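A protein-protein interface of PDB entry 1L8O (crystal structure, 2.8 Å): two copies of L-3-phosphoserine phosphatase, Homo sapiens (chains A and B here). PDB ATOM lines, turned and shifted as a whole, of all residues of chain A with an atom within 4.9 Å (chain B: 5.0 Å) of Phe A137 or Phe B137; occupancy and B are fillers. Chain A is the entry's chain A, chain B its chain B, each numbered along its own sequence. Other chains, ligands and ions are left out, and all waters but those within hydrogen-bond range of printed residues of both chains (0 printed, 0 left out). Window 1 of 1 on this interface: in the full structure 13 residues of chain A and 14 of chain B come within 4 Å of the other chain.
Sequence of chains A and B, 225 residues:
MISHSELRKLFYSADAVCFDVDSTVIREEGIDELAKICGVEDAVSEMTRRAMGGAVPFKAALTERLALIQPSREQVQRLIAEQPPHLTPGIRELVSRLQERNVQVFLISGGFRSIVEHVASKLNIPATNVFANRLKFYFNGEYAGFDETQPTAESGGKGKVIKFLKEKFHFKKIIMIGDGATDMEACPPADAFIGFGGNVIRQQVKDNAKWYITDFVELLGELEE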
ATOM      1  N   PRO A  71      -0.348  -3.473   1.614  1.00  0.00           N
ATOM      2  CA  PRO A  71      -1.007  -2.832   0.479  1.00  0.00           C
ATOM      3  C   PRO A  71      -0.607  -1.375   0.380  1.00  0.00           C
ATOM      4  O   PRO A  71      -0.254  -0.736   1.364  1.00  0.00           O
ATOM      5  CB  PRO A  71      -2.476  -3.003   0.804  1.00  0.00           C
ATOM      6  CG  PRO A  71      -2.493  -2.826   2.280  1.00  0.00           C
ATOM      7  CD  PRO A  71      -1.294  -3.642   2.737  1.00  0.00           C
ATOM      8  N   SER A  72      -0.672  -0.841  -0.819  1.00  0.00           N
ATOM      9  CA  SER A  72      -0.299   0.529  -0.986  1.00  0.00           C
ATOM     10  C   SER A  72      -1.498   1.347  -1.392  1.00  0.00           C
ATOM     11  O   SER A  72      -2.411   0.859  -2.055  1.00  0.00           O
ATOM     12  CB  SER A  72       0.790   0.636  -2.042  1.00  0.00           C
ATOM     13  OG  SER A  72       0.402   0.000  -3.242  1.00  0.00           O
ATOM     14  N   ARG A  73      -1.490   2.604  -0.988  1.00  0.00           N
ATOM     15  CA  ARG A  73      -2.571   3.459  -1.344  1.00  0.00           C
ATOM     16  C   ARG A  73      -2.803   3.257  -2.833  1.00  0.00           C
ATOM     17  O   ARG A  73      -3.930   3.283  -3.290  1.00  0.00           O
ATOM     18  CB  ARG A  73      -2.226   4.909  -1.020  1.00  0.00           C
ATOM     19  CG  ARG A  73      -3.373   5.883  -1.209  1.00  0.00           C
ATOM     20  CD  ARG A  73      -3.477   6.337  -2.648  1.00  0.00           C
ATOM     21  NE  ARG A  73      -4.846   6.666  -3.037  1.00  0.00           N
ATOM     22  CZ  ARG A  73      -5.599   7.575  -2.430  1.00  0.00           C
ATOM     23  NH1 ARG A  73      -5.122   8.259  -1.395  1.00  0.00           N
ATOM     24  NH2 ARG A  73      -6.827   7.799  -2.872  1.00  0.00           N
ATOM     25  N   VAL A  76      -4.283  -0.655  -3.512  1.00  0.00           N
ATOM     26  CA  VAL A  76      -5.712  -0.778  -3.232  1.00  0.00           C
ATOM     27  C   VAL A  76      -6.459   0.127  -4.197  1.00  0.00           C
ATOM     28  O   VAL A  76      -7.544  -0.215  -4.656  1.00  0.00           O
ATOM     29  CB  VAL A  76      -6.130  -0.423  -1.742  1.00  0.00           C
ATOM     30  CG1 VAL A  76      -5.017  -0.746  -0.789  1.00  0.00           C
ATOM     31  CG2 VAL A  76      -6.575   1.017  -1.614  1.00  0.00           C
ATOM     32  N   LEU A 135      -6.976   1.826   6.819  1.00  0.00           N
ATOM     33  CA  LEU A 135      -5.564   1.581   6.616  1.00  0.00           C
ATOM     34  C   LEU A 135      -4.903   2.944   6.519  1.00  0.00           C
ATOM     35  O   LEU A 135      -5.563   3.942   6.213  1.00  0.00           O
ATOM     36  CB  LEU A 135      -5.307   0.773   5.346  1.00  0.00           C
ATOM     37  CG  LEU A 135      -6.514   0.115   4.728  1.00  0.00           C
ATOM     38  CD1 LEU A 135      -7.453   1.198   4.172  1.00  0.00           C
ATOM     39  CD2 LEU A 135      -6.084  -0.816   3.654  1.00  0.00           C
ATOM     40  N   LYS A 136      -3.602   2.957   6.797  1.00  0.00           N
ATOM     41  CA  LYS A 136      -2.772   4.148   6.758  1.00  0.00           C
ATOM     42  C   LYS A 136      -1.707   3.999   5.670  1.00  0.00           C
ATOM     43  O   LYS A 136      -1.197   2.905   5.442  1.00  0.00           O
ATOM     44  CB  LYS A 136      -2.055   4.349   8.096  1.00  0.00           C
ATOM     45  CG  LYS A 136      -2.952   4.623   9.288  1.00  0.00           C
ATOM     46  CD  LYS A 136      -2.112   5.015  10.505  1.00  0.00           C
ATOM     47  CE  LYS A 136      -2.932   5.026  11.791  1.00  0.00           C
ATOM     48  NZ  LYS A 136      -4.174   5.862  11.651  1.00  0.00           N
ATOM     49  N   PHE A 137      -1.364   5.100   5.011  1.00  0.00           N
ATOM     50  CA  PHE A 137      -0.336   5.082   3.973  1.00  0.00           C
ATOM     51  C   PHE A 137       0.594   6.264   4.230  1.00  0.00           C
ATOM     52  O   PHE A 137       0.201   7.204   4.926  1.00  0.00           O
ATOM     53  CB  PHE A 137      -0.987   5.210   2.590  1.00  0.00           C
ATOM     54  CG  PHE A 137      -2.033   4.160   2.315  1.00  0.00           C
ATOM     55  CD1 PHE A 137      -1.661   2.842   2.063  1.00  0.00           C
ATOM     56  CD2 PHE A 137      -3.391   4.476   2.371  1.00  0.00           C
ATOM     57  CE1 PHE A 137      -2.619   1.862   1.878  1.00  0.00           C
ATOM     58  CE2 PHE A 137      -4.355   3.503   2.187  1.00  0.00           C
ATOM     59  CZ  PHE A 137      -3.971   2.194   1.941  1.00  0.00           C
ATOM     60  N   TYR A 138       1.822   6.186   3.695  1.00  0.00           N
ATOM     61  CA  TYR A 138       2.857   7.239   3.788  1.00  0.00           C
ATOM     62  C   TYR A 138       2.742   8.062   2.522  1.00  0.00           C
ATOM     63  O   TYR A 138       2.119   7.627   1.555  1.00  0.00           O
ATOM     64  CB  TYR A 138       4.259   6.644   3.796  1.00  0.00           C
ATOM     65  CG  TYR A 138       4.653   6.001   5.075  1.00  0.00           C
ATOM     66  CD1 TYR A 138       5.212   4.722   5.093  1.00  0.00           C
ATOM     67  CD2 TYR A 138       4.457   6.652   6.283  1.00  0.00           C
ATOM     68  CE1 TYR A 138       5.561   4.106   6.296  1.00  0.00           C
ATOM     69  CE2 TYR A 138       4.804   6.044   7.488  1.00  0.00           C
ATOM     70  CZ  TYR A 138       5.352   4.777   7.488  1.00  0.00           C
ATOM     71  OH  TYR A 138       5.680   4.194   8.675  1.00  0.00           O
ATOM     72  N   PHE A 139       3.354   9.238   2.507  1.00  0.00           N
ATOM     73  CA  PHE A 139       3.306  10.071   1.309  1.00  0.00           C
ATOM     74  C   PHE A 139       3.624   9.195   0.065  1.00  0.00           C
ATOM     75  O   PHE A 139       2.905   9.240  -0.937  1.00  0.00           O
ATOM     76  CB  PHE A 139       4.302  11.243   1.441  1.00  0.00           C
ATOM     77  CG  PHE A 139       3.927  12.457   0.621  1.00  0.00           C
ATOM     78  CD1 PHE A 139       2.735  13.134   0.846  1.00  0.00           C
ATOM     79  CD2 PHE A 139       4.746  12.893  -0.407  1.00  0.00           C
ATOM     80  CE1 PHE A 139       2.377  14.214   0.047  1.00  0.00           C
ATOM     81  CE2 PHE A 139       4.388  13.971  -1.201  1.00  0.00           C
ATOM     82  CZ  PHE A 139       3.205  14.630  -0.975  1.00  0.00           C
ATOM     83  N   GLY A 141       3.117   6.312  -0.347  1.00  0.00           N
ATOM     84  CA  GLY A 141       1.990   5.421  -0.551  1.00  0.00           C
ATOM     85  C   GLY A 141       2.241   4.047   0.035  1.00  0.00           C
ATOM     86  O   GLY A 141       1.410   3.162  -0.095  1.00  0.00           O
ATOM     87  N   GLU A 142       3.393   3.861   0.668  1.00  0.00           N
ATOM     88  CA  GLU A 142       3.711   2.572   1.248  1.00  0.00           C
ATOM     89  C   GLU A 142       2.726   2.259   2.385  1.00  0.00           C
ATOM     90  O   GLU A 142       2.036   3.150   2.895  1.00  0.00           O
ATOM     91  CB  GLU A 142       5.138   2.557   1.810  1.00  0.00           C
ATOM     92  CG  GLU A 142       6.303   2.194   0.868  1.00  0.00           C
ATOM     93  CD  GLU A 142       7.576   1.834   1.667  1.00  0.00           C
ATOM     94  OE1 GLU A 142       8.117   2.716   2.375  1.00  0.00           O
ATOM     95  OE2 GLU A 142       8.013   0.663   1.601  1.00  0.00           O
ATOM     96  N   TYR A 143       2.662   0.989   2.778  1.00  0.00           N
ATOM     97  CA  TYR A 143       1.774   0.589   3.847  1.00  0.00           C
ATOM     98  C   TYR A 143       2.323   1.128   5.161  1.00  0.00           C
ATOM     99  O   TYR A 143       3.531   1.176   5.342  1.00  0.00           O
ATOM    100  CB  TYR A 143       1.662  -0.934   3.899  1.00  0.00           C
ATOM    101  CG  TYR A 143       1.007  -1.464   5.156  1.00  0.00           C
ATOM    102  CD1 TYR A 143      -0.289  -1.099   5.500  1.00  0.00           C
ATOM    103  CD2 TYR A 143       1.703  -2.340   6.005  1.00  0.00           C
ATOM    104  CE1 TYR A 143      -0.883  -1.591   6.654  1.00  0.00           C
ATOM    105  CE2 TYR A 143       1.129  -2.841   7.157  1.00  0.00           C
ATOM    106  CZ  TYR A 143      -0.177  -2.466   7.485  1.00  0.00           C
ATOM    107  OH  TYR A 143      -0.773  -2.998   8.622  1.00  0.00           O
ATOM    108  N   ALA A 144       1.437   1.533   6.071  1.00  0.00           N
ATOM    109  CA  ALA A 144       1.849   2.066   7.371  1.00  0.00           C
ATOM    110  C   ALA A 144       1.253   1.263   8.522  1.00  0.00           C
ATOM    111  O   ALA A 144       1.946   0.935   9.496  1.00  0.00           O
ATOM    112  CB  ALA A 144       1.434   3.512   7.497  1.00  0.00           C
ATOM    113  N   PRO B  71      -2.499  17.663   9.490  1.00  0.00           N
ATOM    114  CA  PRO B  71      -2.358  17.924   8.059  1.00  0.00           C
ATOM    115  C   PRO B  71      -2.818  16.801   7.131  1.00  0.00           C
ATOM    116  O   PRO B  71      -2.576  15.626   7.391  1.00  0.00           O
ATOM    117  CB  PRO B  71      -0.866  18.213   7.924  1.00  0.00           C
ATOM    118  CG  PRO B  71      -0.271  17.281   8.923  1.00  0.00           C
ATOM    119  CD  PRO B  71      -1.186  17.415  10.116  1.00  0.00           C
ATOM    120  N   SER B  72      -3.482  17.169   6.042  1.00  0.00           N
ATOM    121  CA  SER B  72      -3.959  16.185   5.084  1.00  0.00           C
ATOM    122  C   SER B  72      -2.963  15.954   3.955  1.00  0.00           C
ATOM    123  O   SER B  72      -2.193  16.839   3.608  1.00  0.00           O
ATOM    124  CB  SER B  72      -5.316  16.630   4.510  1.00  0.00           C
ATOM    125  OG  SER B  72      -5.226  17.573   3.447  1.00  0.00           O
ATOM    126  N   ARG B  73      -2.964  14.761   3.381  1.00  0.00           N
ATOM    127  CA  ARG B  73      -2.050  14.489   2.286  1.00  0.00           C
ATOM    128  C   ARG B  73      -2.213  15.614   1.266  1.00  0.00           C
ATOM    129  O   ARG B  73      -1.241  16.148   0.784  1.00  0.00           O
ATOM    130  CB  ARG B  73      -2.369  13.128   1.659  1.00  0.00           C
ATOM    131  CG  ARG B  73      -1.711  12.868   0.315  1.00  0.00           C
ATOM    132  CD  ARG B  73      -2.554  11.937  -0.560  1.00  0.00           C
ATOM    133  NE  ARG B  73      -1.967  10.608  -0.655  1.00  0.00           N
ATOM    134  CZ  ARG B  73      -0.760  10.372  -1.147  1.00  0.00           C
ATOM    135  NH1 ARG B  73      -0.024  11.388  -1.593  1.00  0.00           N
ATOM    136  NH2 ARG B  73      -0.288   9.130  -1.175  1.00  0.00           N
ATOM    137  N   VAL B  76      -0.144  18.618   2.308  1.00  0.00           N
ATOM    138  CA  VAL B  76       1.274  18.406   2.056  1.00  0.00           C
ATOM    139  C   VAL B  76       1.610  18.297   0.561  1.00  0.00           C
ATOM    140  O   VAL B  76       2.715  18.620   0.149  1.00  0.00           O
ATOM    141  CB  VAL B  76       1.772  17.134   2.755  1.00  0.00           C
ATOM    142  CG1 VAL B  76       3.229  16.931   2.493  1.00  0.00           C
ATOM    143  CG2 VAL B  76       1.515  17.236   4.248  1.00  0.00           C
ATOM    144  N   LEU B 135       5.235  11.076   7.758  1.00  0.00           N
ATOM    145  CA  LEU B 135       3.840  11.376   8.042  1.00  0.00           C
ATOM    146  C   LEU B 135       2.939  10.246   7.517  1.00  0.00           C
ATOM    147  O   LEU B 135       3.200   9.671   6.459  1.00  0.00           O
ATOM    148  CB  LEU B 135       3.433  12.697   7.395  1.00  0.00           C
ATOM    149  CG  LEU B 135       3.892  13.957   8.127  1.00  0.00           C
ATOM    150  CD1 LEU B 135       3.219  15.198   7.514  1.00  0.00           C
ATOM    151  CD2 LEU B 135       3.523  13.849   9.592  1.00  0.00           C
ATOM    152  N   LYS B 136       1.883   9.941   8.272  1.00  0.00           N
ATOM    153  CA  LYS B 136       0.942   8.879   7.932  1.00  0.00           C
ATOM    154  C   LYS B 136      -0.379   9.477   7.474  1.00  0.00           C
ATOM    155  O   LYS B 136      -0.761  10.545   7.951  1.00  0.00           O
ATOM    156  CB  LYS B 136       0.720   7.984   9.158  1.00  0.00           C
ATOM    157  CG  LYS B 136       1.880   7.041   9.475  1.00  0.00           C
ATOM    158  CD  LYS B 136       1.875   6.530  10.910  1.00  0.00           C
ATOM    159  CE  LYS B 136       2.749   5.297  11.038  1.00  0.00           C
ATOM    160  NZ  LYS B 136       3.202   4.971  12.430  1.00  0.00           N
ATOM    161  N   PHE B 137      -1.076   8.798   6.560  1.00  0.00           N
ATOM    162  CA  PHE B 137      -2.367   9.295   6.061  1.00  0.00           C
ATOM    163  C   PHE B 137      -3.367   8.163   5.803  1.00  0.00           C
ATOM    164  O   PHE B 137      -2.961   7.018   5.610  1.00  0.00           O
ATOM    165  CB  PHE B 137      -2.164  10.077   4.759  1.00  0.00           C
ATOM    166  CG  PHE B 137      -1.373  11.337   4.922  1.00  0.00           C
ATOM    167  CD1 PHE B 137      -1.917  12.430   5.574  1.00  0.00           C
ATOM    168  CD2 PHE B 137      -0.061  11.417   4.451  1.00  0.00           C
ATOM    169  CE1 PHE B 137      -1.168  13.581   5.759  1.00  0.00           C
ATOM    170  CE2 PHE B 137       0.701  12.565   4.631  1.00  0.00           C
ATOM    171  CZ  PHE B 137       0.153  13.649   5.284  1.00  0.00           C
ATOM    172  N   TYR B 138      -4.665   8.478   5.807  1.00  0.00           N
ATOM    173  CA  TYR B 138      -5.688   7.467   5.522  1.00  0.00           C
ATOM    174  C   TYR B 138      -5.977   7.516   4.026  1.00  0.00           C
ATOM    175  O   TYR B 138      -5.866   8.575   3.420  1.00  0.00           O
ATOM    176  CB  TYR B 138      -6.993   7.737   6.271  1.00  0.00           C
ATOM    177  CG  TYR B 138      -6.930   7.487   7.753  1.00  0.00           C
ATOM    178  CD1 TYR B 138      -7.411   8.429   8.639  1.00  0.00           C
ATOM    179  CD2 TYR B 138      -6.352   6.338   8.270  1.00  0.00           C
ATOM    180  CE1 TYR B 138      -7.323   8.254  10.005  1.00  0.00           C
ATOM    181  CE2 TYR B 138      -6.254   6.145   9.649  1.00  0.00           C
ATOM    182  CZ  TYR B 138      -6.741   7.118  10.510  1.00  0.00           C
ATOM    183  OH  TYR B 138      -6.620   6.987  11.875  1.00  0.00           O
ATOM    184  N   PHE B 139      -6.338   6.371   3.441  1.00  0.00           N
ATOM    185  CA  PHE B 139      -6.643   6.273   2.012  1.00  0.00           C
ATOM    186  C   PHE B 139      -7.628   7.359   1.635  1.00  0.00           C
ATOM    187  O   PHE B 139      -7.888   7.632   0.473  1.00  0.00           O
ATOM    188  CB  PHE B 139      -7.268   4.910   1.682  1.00  0.00           C
ATOM    189  CG  PHE B 139      -7.844   4.836   0.299  1.00  0.00           C
ATOM    190  CD1 PHE B 139      -7.045   4.525  -0.784  1.00  0.00           C
ATOM    191  CD2 PHE B 139      -9.177   5.164   0.067  1.00  0.00           C
ATOM    192  CE1 PHE B 139      -7.568   4.546  -2.094  1.00  0.00           C
ATOM    193  CE2 PHE B 139      -9.710   5.190  -1.237  1.00  0.00           C
ATOM    194  CZ  PHE B 139      -8.903   4.883  -2.313  1.00  0.00           C
ATOM    195  N   GLY B 141      -7.055  10.234   2.539  1.00  0.00           N
ATOM    196  CA  GLY B 141      -6.157  11.387   2.576  1.00  0.00           C
ATOM    197  C   GLY B 141      -6.358  12.239   3.820  1.00  0.00           C
ATOM    198  O   GLY B 141      -6.705  13.397   3.669  1.00  0.00           O
ATOM    199  N   GLU B 142      -6.132  11.686   5.019  1.00  0.00           N
ATOM    200  CA  GLU B 142      -6.338  12.401   6.281  1.00  0.00           C
ATOM    201  C   GLU B 142      -5.315  12.037   7.356  1.00  0.00           C
ATOM    202  O   GLU B 142      -5.052  10.853   7.578  1.00  0.00           O
ATOM    203  CB  GLU B 142      -7.704  12.068   6.869  1.00  0.00           C
ATOM    204  CG  GLU B 142      -8.902  12.258   5.937  1.00  0.00           C
ATOM    205  CD  GLU B 142     -10.184  11.544   6.412  1.00  0.00           C
ATOM    206  OE1 GLU B 142     -10.794  10.863   5.539  1.00  0.00           O
ATOM    207  OE2 GLU B 142     -10.567  11.664   7.617  1.00  0.00           O
ATOM    208  N   TYR B 143      -4.775  13.033   8.063  1.00  0.00           N
ATOM    209  CA  TYR B 143      -3.774  12.775   9.110  1.00  0.00           C
ATOM    210  C   TYR B 143      -4.087  11.558   9.978  1.00  0.00           C
ATOM    211  O   TYR B 143      -5.154  11.481  10.582  1.00  0.00           O
ATOM    212  CB  TYR B 143      -3.615  13.999  10.020  1.00  0.00           C
ATOM    213  CG  TYR B 143      -2.553  13.781  11.065  1.00  0.00           C
ATOM    214  CD1 TYR B 143      -1.294  13.335  10.682  1.00  0.00           C
ATOM    215  CD2 TYR B 143      -2.820  13.929  12.428  1.00  0.00           C
ATOM    216  CE1 TYR B 143      -0.329  13.022  11.609  1.00  0.00           C
ATOM    217  CE2 TYR B 143      -1.842  13.621  13.395  1.00  0.00           C
ATOM    218  CZ  TYR B 143      -0.598  13.155  12.966  1.00  0.00           C
ATOM    219  OH  TYR B 143       0.391  12.751  13.844  1.00  0.00           O
ATOM    220  N   ALA B 144      -3.128  10.630  10.038  1.00  0.00           N
ATOM    221  CA  ALA B 144      -3.192   9.367  10.803  1.00  0.00           C
ATOM    222  C   ALA B 144      -1.980   9.175  11.719  1.00  0.00           C
ATOM    223  O   ALA B 144      -1.635   8.036  12.074  1.00  0.00           O
ATOM    224  CB  ALA B 144      -3.259   8.195   9.845  1.00  0.00           C
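Leu A135 touches Tyr B138. Leu A135 touches Phe B139. Lys A136 touches Phe B137. Phe A137 touches Lys B136 (O to C, 3.5 Å). Phe B139 touches Phe A137 (CB to CE2, 3.3 Å). Arg B73 touches Tyr A138 (NH2 to O, 3.9 Å). Tyr A138 touches Leu B135 (CD2 to O, 3.3 Å). CE2 of Tyr A138 touches CG of Lys B136 (3.7 Å). Phe A139 touches Val B76 (CE1 to CG1, 3.8 Å). N of Phe A139 touches O of Leu B135, 3.98 Å away.
Of the 13 printed residues of chain B, 8 touch a printed residue of chain A. Hydrophobic or aromatic side chains of chain B that line the printed part of chain A: Val B76, Phe B137, Tyr B138, Phe B139 and Ala B144. Among the printed residues, 16 pairs touch across the chains. Among the printed residues, no Asp or Glu carboxylate lies within 4 Å of a Lys or Arg side-chain nitrogen of the other chain.
The backbone carbonyl oxygen of Phe B139 lies within hydrogen-bond range of the guanidinium group of Arg A73. The side-chain hydroxyl of Tyr B138 is in hydrogen-bond range of the side-chain amino group of Lys A136, at 2.7 Å. NZ of Lys A136 sits close to O of Ala B144 (3.4 Å). O of Phe B137 lies within hydrogen-bond range of N of Phe A137, at 2.6 Å. NH2 of Arg B73 lies within hydrogen-bond range of O of Phe A139, 3.2 Å away.
Leu A135 touches Tyr B138, and with the chains exchanged Tyr A138 touches Leu B135. Leu A135 touches Phe B139, and with the chains exchanged Phe A139 touches Leu B135. Lys A136 touches Phe B137, and with the chains exchanged Phe A137 touches Lys B136. Tyr A138 touches Arg B73, but with the chains exchanged Arg A73 does not touch Tyr B138 (4.9 Å).
N of Arg A73 is in hydrogen-bond range of O of Gly A141 (3.1 Å). The backbone carbonyl oxygen (O) of Lys A136 is in hydrogen-bond range of the backbone NH (N) of Ala A144. The backbone carbonyl oxygen of Lys B136 sits at hydrogen-bond distance from the backbone NH of Ala B144, at 3.2 Å.
Of the printed residues of chain B, Lys A136 touches Phe B137, Tyr B138 and Ala B144. Phe A137 touches three residues of chain B. Of the printed residues of chain B, Phe A139 touches Arg B73 (3.2 Å), Val B76 (3.8 Å) and Leu B135 (3.98 Å). Pro B71 touches none of the printed residues of chain A. Of the printed residues of chain A, Lys B136 touches Phe A137 and Tyr A138. Phe B137 touches just these residues of chain A: Lys A136 and Phe A137. Of the printed residues of chain A, Tyr B138 touches Leu A135 and Lys A136. Of the printed residues of chain A, Phe B139 touches Arg A73 (3.4 Å), Val A76 (3.6 Å), Leu A135 (3.8 Å) and Phe A137 (3.3 Å). Tyr B143 touches none of the printed residues of chain A. The nearest printed residue of chain A that does not touch Lys B136 is Ala A144 (4.1 Å).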
